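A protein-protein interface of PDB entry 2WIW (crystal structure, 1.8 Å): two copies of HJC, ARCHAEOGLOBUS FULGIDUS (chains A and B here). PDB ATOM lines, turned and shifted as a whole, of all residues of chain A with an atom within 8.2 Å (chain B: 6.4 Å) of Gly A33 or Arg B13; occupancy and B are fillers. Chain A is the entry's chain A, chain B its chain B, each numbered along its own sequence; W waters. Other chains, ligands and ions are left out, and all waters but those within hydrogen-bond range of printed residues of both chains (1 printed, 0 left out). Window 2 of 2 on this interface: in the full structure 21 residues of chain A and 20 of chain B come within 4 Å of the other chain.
The backbone carbonyl oxygen (O) of Gly A31 is in hydrogen-bond range of the backbone NH (N) of Arg B28 (2.8 Å). The backbone carbonyl oxygen (O) of Arg B28 lies within hydrogen-bond range of the backbone NH (N) of Ala A30, 3.0 Å away. The guanidinium group (NH1) of Arg B13 is in hydrogen-bond range of the backbone carbonyl oxygen (O) of Gly A33 (3.1 Å).
The side-chain carboxylate (OE1) of Glu B12 lies within salt-bridge range of the guanidinium group (NE) of Arg B28, 3.1 Å away. The backbone NH of Ser A35 sits at hydrogen-bond distance from the side-chain hydroxyl of Ser A32, at 3.4 Å. The side-chain hydroxyl (OG) of Ser A32 lies close to the backbone NH (N) of Val A34, at 3.4 Å.
Among the printed residues, merely in contact across the chains: Ser A32 with Ala B26 (3.4 Å), Ser A32 with Leu B16 (3.5 Å), Gly A33 with Leu B16 (3.7 Å) and Val A29 with Arg B28 (3.9 Å).
Gly A33 touches just these residues of chain B: Arg B13 (3.1 Å) and Leu B16 (3.7 Å). Arg B13 touches one residue of chain A. Of the printed residues of chain A, Arg B28 touches Val A29, Ala A30 and Gly A31. Of the printed residues of chain A, Leu B16 touches Ser A32 and Gly A33. Of the printed residues of chain B, Ser A32 touches Leu B16 and Ala B26. Of the printed residues of chain B, Gly A31 touches Arg B28. Arg B10 touches none of the printed residues of chain A. Glu B12 touches none of the printed residues of chain A. The nearest residue of chain B that does not touch Gly A33 is Val B17 (4.2 Å). The nearest residue of chain A that does not touch Arg B13 is Val A34 (5.1 Å). The nearest printed residue of chain B that does not touch Gly A31 is Ala B26 (4.3 Å).
Hydrophobic or aromatic side chains of chain A that line the printed part of chain B: Ala A30. Along chain A the printed residues that touch a printed residue of chain B span positions 29 to 33. Printed residues of chain B that touch a printed residue of chain A: Arg B13, Leu B16, Ala B26 and Arg B28. Hydrophobic or aromatic side chains of chain B that line the printed part of chain A: Leu B16. Among the printed residues, no Asp or Glu carboxylate lies within 4 Å of a Lys or Arg side-chain nitrogen of the other chain.
No position is printed for both chains. Of the 7 pairs that touch across the chains among the printed residues, none has its exchanged pair printed and touching as well.
Water W1 lies within hydrogen-bond range of O of Leu B16 (2.7 Å) and O of Ser A32 (2.8 Å).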
ATOM      1  N   VAL A  29      10.170  25.879 -13.286  1.00  0.00           N
ATOM      2  CA  VAL A  29      10.011  24.919 -12.206  1.00  0.00           C
ATOM      3  C   VAL A  29       8.973  25.355 -11.196  1.00  0.00           C
ATOM      4  O   VAL A  29       9.030  26.476 -10.693  1.00  0.00           O
ATOM      5  CB  VAL A  29      11.360  24.768 -11.461  1.00  0.00           C
ATOM      6  CG1 VAL A  29      11.214  23.870 -10.242  1.00  0.00           C
ATOM      7  CG2 VAL A  29      12.432  24.274 -12.434  1.00  0.00           C
ATOM      8  N   ALA A  30       8.035  24.466 -10.878  1.00  0.00           N
ATOM      9  CA  ALA A  30       7.079  24.722  -9.805  1.00  0.00           C
ATOM     10  C   ALA A  30       7.588  24.211  -8.453  1.00  0.00           C
ATOM     11  O   ALA A  30       7.361  24.841  -7.419  1.00  0.00           O
ATOM     12  CB  ALA A  30       5.732  24.095 -10.136  1.00  0.00           C
ATOM     13  N   GLY A  31       8.278  23.076  -8.457  1.00  0.00           N
ATOM     14  CA  GLY A  31       8.758  22.476  -7.218  1.00  0.00           C
ATOM     15  C   GLY A  31       9.198  21.033  -7.400  1.00  0.00           C
ATOM     16  O   GLY A  31       9.072  20.495  -8.495  1.00  0.00           O
ATOM     17  N   SER A  32       9.701  20.410  -6.329  1.00  0.00           N
ATOM     18  CA  SER A  32      10.233  19.045  -6.380  1.00  0.00           C
ATOM     19  C   SER A  32       9.490  18.066  -5.453  1.00  0.00           C
ATOM     20  O   SER A  32       9.847  16.879  -5.369  1.00  0.00           O
ATOM     21  CB  SER A  32      11.698  19.047  -5.969  1.00  0.00           C
ATOM     22  OG  SER A  32      11.790  19.015  -4.557  1.00  0.00           O
ATOM     23  N   GLY A  33       8.490  18.568  -4.733  1.00  0.00           N
ATOM     24  CA  GLY A  33       7.666  17.729  -3.878  1.00  0.00           C
ATOM     25  C   GLY A  33       8.298  17.321  -2.560  1.00  0.00           C
ATOM     26  O   GLY A  33       7.600  16.853  -1.663  1.00  0.00           O
ATOM     27  N   VAL A  34       9.610  17.492  -2.433  1.00  0.00           N
ATOM     28  CA  VAL A  34      10.325  17.062  -1.229  1.00  0.00           C
ATOM     29  C   VAL A  34      10.941  18.236  -0.462  1.00  0.00           C
ATOM     30  O   VAL A  34      11.097  18.174   0.755  1.00  0.00           O
ATOM     31  CB  VAL A  34      11.434  16.043  -1.566  1.00  0.00           C
ATOM     32  CG1 VAL A  34      10.828  14.743  -2.084  1.00  0.00           C
ATOM     33  CG2 VAL A  34      12.410  16.627  -2.579  1.00  0.00           C
ATOM     34  N   SER A  35      11.286  19.302  -1.175  1.00  0.00           N
ATOM     35  CA  SER A  35      11.881  20.475  -0.547  1.00  0.00           C
ATOM     36  C   SER A  35      10.835  21.567  -0.346  1.00  0.00           C
ATOM     37  O   SER A  35       9.845  21.624  -1.077  1.00  0.00           O
ATOM     38  CB  SER A  35      13.032  21.011  -1.403  1.00  0.00           C
ATOM     39  OG  SER A  35      13.742  22.030  -0.722  1.00  0.00           O
ATOM     40  N   PRO A  36      11.050  22.436   0.654  1.00  0.00           N
ATOM     41  CA  PRO A  36      10.132  23.555   0.897  1.00  0.00           C
ATOM     42  C   PRO A  36      10.271  24.646  -0.162  1.00  0.00           C
ATOM     43  O   PRO A  36       9.352  25.443  -0.352  1.00  0.00           O
ATOM     44  CB  PRO A  36      10.576  24.092   2.266  1.00  0.00           C
ATOM     45  CG  PRO A  36      11.499  23.052   2.836  1.00  0.00           C
ATOM     46  CD  PRO A  36      12.119  22.379   1.663  1.00  0.00           C
ATOM     47  N   PHE A  37      11.415  24.670  -0.842  1.00  0.00           N
ATOM     48  CA  PHE A  37      11.708  25.710  -1.823  1.00  0.00           C
ATOM     49  C   PHE A  37      11.857  25.130  -3.228  1.00  0.00           C
ATOM     50  O   PHE A  37      12.503  24.098  -3.400  1.00  0.00           O
ATOM     51  CB  PHE A  37      12.995  26.441  -1.434  1.00  0.00           C
ATOM     52  CG  PHE A  37      12.976  26.998  -0.040  1.00  0.00           C
ATOM     53  CD1 PHE A  37      12.268  28.152   0.247  1.00  0.00           C
ATOM     54  CD2 PHE A  37      13.663  26.366   0.982  1.00  0.00           C
ATOM     55  CE1 PHE A  37      12.246  28.667   1.529  1.00  0.00           C
ATOM     56  CE2 PHE A  37      13.645  26.877   2.265  1.00  0.00           C
ATOM     57  CZ  PHE A  37      12.935  28.029   2.539  1.00  0.00           C
ATOM     58  N   PRO A  38      11.247  25.790  -4.234  1.00  0.00           N
ATOM     59  CA  PRO A  38      11.420  25.436  -5.650  1.00  0.00           C
ATOM     60  C   PRO A  38      12.814  25.785  -6.164  1.00  0.00           C
ATOM     61  O   PRO A  38      13.266  26.923  -6.035  1.00  0.00           O
ATOM     62  CB  PRO A  38      10.374  26.300  -6.371  1.00  0.00           C
ATOM     63  CG  PRO A  38       9.439  26.771  -5.316  1.00  0.00           C
ATOM     64  CD  PRO A  38      10.237  26.846  -4.055  1.00  0.00           C
ATOM     65  N   GLY B   8      -0.302  20.461  -5.286  1.00  0.00           N
ATOM     66  CA  GLY B   8      -1.175  19.499  -5.936  1.00  0.00           C
ATOM     67  C   GLY B   8      -0.856  19.356  -7.414  1.00  0.00           C
ATOM     68  O   GLY B   8      -0.053  20.124  -7.949  1.00  0.00           O
ATOM     69  N   THR B   9      -1.463  18.375  -8.081  1.00  0.00           N
ATOM     70  CA  THR B   9      -2.359  17.418  -7.439  1.00  0.00           C
ATOM     71  C   THR B   9      -1.592  16.596  -6.411  1.00  0.00           C
ATOM     72  O   THR B   9      -0.361  16.590  -6.401  1.00  0.00           O
ATOM     73  CB  THR B   9      -2.979  16.447  -8.469  1.00  0.00           C
ATOM     74  OG1 THR B   9      -1.947  15.655  -9.070  1.00  0.00           O
ATOM     75  CG2 THR B   9      -3.716  17.208  -9.559  1.00  0.00           C
ATOM     76  N   ARG B  10      -2.312  15.906  -5.538  1.00  0.00           N
ATOM     77  CA  ARG B  10      -1.652  15.056  -4.560  1.00  0.00           C
ATOM     78  C   ARG B  10      -1.006  13.880  -5.280  1.00  0.00           C
ATOM     79  O   ARG B  10      -0.145  13.209  -4.723  1.00  0.00           O
ATOM     80  CB  ARG B  10      -2.638  14.539  -3.512  1.00  0.00           C
ATOM     81  CG  ARG B  10      -2.921  13.041  -3.620  1.00  0.00           C
ATOM     82  CD  ARG B  10      -3.929  12.559  -2.586  1.00  0.00           C
ATOM     83  NE  ARG B  10      -3.782  13.234  -1.297  1.00  0.00           N
ATOM     84  CZ  ARG B  10      -4.019  12.666  -0.117  1.00  0.00           C
ATOM     85  NH1 ARG B  10      -4.399  11.396  -0.043  1.00  0.00           N
ATOM     86  NH2 ARG B  10      -3.860  13.368   0.996  1.00  0.00           N
ATOM     87  N   PHE B  11      -1.437  13.627  -6.515  1.00  0.00           N
ATOM     88  CA  PHE B  11      -0.902  12.519  -7.297  1.00  0.00           C
ATOM     89  C   PHE B  11       0.501  12.825  -7.760  1.00  0.00           C
ATOM     90  O   PHE B  11       1.383  11.987  -7.657  1.00  0.00           O
ATOM     91  CB  PHE B  11      -1.766  12.241  -8.528  1.00  0.00           C
ATOM     92  CG  PHE B  11      -3.176  11.878  -8.203  1.00  0.00           C
ATOM     93  CD1 PHE B  11      -3.449  10.938  -7.223  1.00  0.00           C
ATOM     94  CD2 PHE B  11      -4.227  12.469  -8.879  1.00  0.00           C
ATOM     95  CE1 PHE B  11      -4.749  10.600  -6.917  1.00  0.00           C
ATOM     96  CE2 PHE B  11      -5.531  12.134  -8.581  1.00  0.00           C
ATOM     97  CZ  PHE B  11      -5.794  11.196  -7.599  1.00  0.00           C
ATOM     98  N   GLU B  12       0.696  14.018  -8.312  1.00  0.00           N
ATOM     99  CA  GLU B  12       2.017  14.436  -8.773  1.00  0.00           C
ATOM    100  C   GLU B  12       2.981  14.475  -7.603  1.00  0.00           C
ATOM    101  O   GLU B  12       4.125  14.055  -7.721  1.00  0.00           O
ATOM    102  CB  GLU B  12       1.945  15.808  -9.441  1.00  0.00           C
ATOM    103  CG  GLU B  12       1.507  15.743 -10.894  1.00  0.00           C
ATOM    104  CD  GLU B  12       0.716  16.960 -11.327  1.00  0.00           C
ATOM    105  OE1 GLU B  12       0.449  17.842 -10.477  1.00  0.00           O
ATOM    106  OE2 GLU B  12       0.355  17.027 -12.519  1.00  0.00           O
ATOM    107  N   ARG B  13       2.502  14.982  -6.473  1.00  0.00           N
ATOM    108  CA  ARG B  13       3.306  15.085  -5.262  1.00  0.00           C
ATOM    109  C   ARG B  13       3.846  13.713  -4.847  1.00  0.00           C
ATOM    110  O   ARG B  13       5.039  13.560  -4.580  1.00  0.00           O
ATOM    111  CB  ARG B  13       2.463  15.714  -4.143  1.00  0.00           C
ATOM    112  CG  ARG B  13       2.757  15.211  -2.738  1.00  0.00           C
ATOM    113  CD  ARG B  13       3.764  16.079  -2.006  1.00  0.00           C
ATOM    114  NE  ARG B  13       3.940  15.645  -0.620  1.00  0.00           N
ATOM    115  CZ  ARG B  13       4.584  16.341   0.312  1.00  0.00           C
ATOM    116  NH1 ARG B  13       5.120  17.520   0.021  1.00  0.00           N
ATOM    117  NH2 ARG B  13       4.688  15.858   1.543  1.00  0.00           N
ATOM    118  N   ASP B  14       2.958  12.724  -4.796  1.00  0.00           N
ATOM    119  CA  ASP B  14       3.307  11.377  -4.365  1.00  0.00           C
ATOM    120  C   ASP B  14       4.310  10.736  -5.321  1.00  0.00           C
ATOM    121  O   ASP B  14       5.200  10.001  -4.895  1.00  0.00           O
ATOM    122  CB  ASP B  14       2.053  10.509  -4.293  1.00  0.00           C
ATOM    123  CG  ASP B  14       2.364   9.075  -3.931  1.00  0.00           C
ATOM    124  OD1 ASP B  14       3.018   8.860  -2.889  1.00  0.00           O
ATOM    125  OD2 ASP B  14       1.959   8.163  -4.683  1.00  0.00           O
ATOM    126  N   LEU B  15       4.149  11.005  -6.614  1.00  0.00           N
ATOM    127  CA  LEU B  15       5.072  10.514  -7.621  1.00  0.00           C
ATOM    128  C   LEU B  15       6.435  11.222  -7.498  1.00  0.00           C
ATOM    129  O   LEU B  15       7.475  10.616  -7.707  1.00  0.00           O
ATOM    130  CB  LEU B  15       4.496  10.737  -9.024  1.00  0.00           C
ATOM    131  CG  LEU B  15       5.441  10.368 -10.165  1.00  0.00           C
ATOM    132  CD1 LEU B  15       5.885   8.938 -10.030  1.00  0.00           C
ATOM    133  CD2 LEU B  15       4.754  10.576 -11.534  1.00  0.00           C
ATOM    134  N   LEU B  16       6.424  12.504  -7.161  1.00  0.00           N
ATOM    135  CA  LEU B  16       7.687  13.220  -6.972  1.00  0.00           C
ATOM    136  C   LEU B  16       8.452  12.590  -5.808  1.00  0.00           C
ATOM    137  O   LEU B  16       9.674  12.453  -5.871  1.00  0.00           O
ATOM    138  CB  LEU B  16       7.453  14.711  -6.699  1.00  0.00           C
ATOM    139  CG  LEU B  16       6.970  15.548  -7.893  1.00  0.00           C
ATOM    140  CD1 LEU B  16       6.527  16.899  -7.405  1.00  0.00           C
ATOM    141  CD2 LEU B  16       8.066  15.695  -8.965  1.00  0.00           C
ATOM    142  N   VAL B  17       7.746  12.203  -4.748  1.00  0.00           N
ATOM    143  CA  VAL B  17       8.416  11.558  -3.599  1.00  0.00           C
ATOM    144  C   VAL B  17       9.018  10.209  -3.983  1.00  0.00           C
ATOM    145  O   VAL B  17      10.157   9.906  -3.621  1.00  0.00           O
ATOM    146  CB  VAL B  17       7.484  11.349  -2.394  1.00  0.00           C
ATOM    147  CG1 VAL B  17       8.239  10.612  -1.270  1.00  0.00           C
ATOM    148  CG2 VAL B  17       6.951  12.676  -1.882  1.00  0.00           C
ATOM    149  N   GLU B  18       8.268   9.407  -4.743  1.00  0.00           N
ATOM    150  CA  GLU B  18       8.784   8.118  -5.223  1.00  0.00           C
ATOM    151  C   GLU B  18       9.997   8.307  -6.138  1.00  0.00           C
ATOM    152  O   GLU B  18      10.951   7.540  -6.069  1.00  0.00           O
ATOM    153  CB  GLU B  18       7.695   7.317  -5.947  1.00  0.00           C
ATOM    154  CG  GLU B  18       6.497   6.955  -5.068  1.00  0.00           C
ATOM    155  CD  GLU B  18       6.883   6.335  -3.716  1.00  0.00           C
ATOM    156  OE1 GLU B  18       7.605   5.310  -3.683  1.00  0.00           O
ATOM    157  OE2 GLU B  18       6.443   6.872  -2.674  1.00  0.00           O
ATOM    158  N   ALA B  26      13.869  15.404  -9.553  1.00  0.00           N
ATOM    159  CA  ALA B  26      12.646  15.552 -10.368  1.00  0.00           C
ATOM    160  C   ALA B  26      11.959  16.873 -10.040  1.00  0.00           C
ATOM    161  O   ALA B  26      12.046  17.380  -8.912  1.00  0.00           O
ATOM    162  CB  ALA B  26      11.694  14.402 -10.117  1.00  0.00           C
ATOM    163  N   ARG B  28       8.237  19.248 -10.888  1.00  0.00           N
ATOM    164  CA  ARG B  28       6.939  19.531 -11.498  1.00  0.00           C
ATOM    165  C   ARG B  28       7.079  20.783 -12.374  1.00  0.00           C
ATOM    166  O   ARG B  28       7.734  21.734 -11.993  1.00  0.00           O
ATOM    167  CB  ARG B  28       5.899  19.729 -10.386  1.00  0.00           C
ATOM    168  CG  ARG B  28       4.478  20.012 -10.847  1.00  0.00           C
ATOM    169  CD  ARG B  28       3.929  18.894 -11.717  1.00  0.00           C
ATOM    170  NE  ARG B  28       2.589  19.190 -12.232  1.00  0.00           N
ATOM    171  CZ  ARG B  28       2.337  19.817 -13.381  1.00  0.00           C
ATOM    172  NH1 ARG B  28       3.330  20.232 -14.151  1.00  0.00           N
ATOM    173  NH2 ARG B  28       1.085  20.035 -13.766  1.00  0.00           N
ATOM    174  N   ILE B  42       6.167  16.353 -15.547  1.00  0.00           N
ATOM    175  CA  ILE B  42       7.377  16.248 -14.717  1.00  0.00           C
ATOM    176  C   ILE B  42       8.584  16.023 -15.613  1.00  0.00           C
ATOM    177  O   ILE B  42       8.495  15.410 -16.681  1.00  0.00           O
ATOM    178  CB  ILE B  42       7.255  15.103 -13.688  1.00  0.00           C
ATOM    179  CG1 ILE B  42       6.189  15.433 -12.629  1.00  0.00           C
ATOM    180  CG2 ILE B  42       8.603  14.811 -12.995  1.00  0.00           C
ATOM    181  CD1 ILE B  42       5.930  14.246 -11.674  1.00  0.00           C
HETATM  182  O   HOH W   1      11.181  14.623  -6.360  1.00  0.00           O
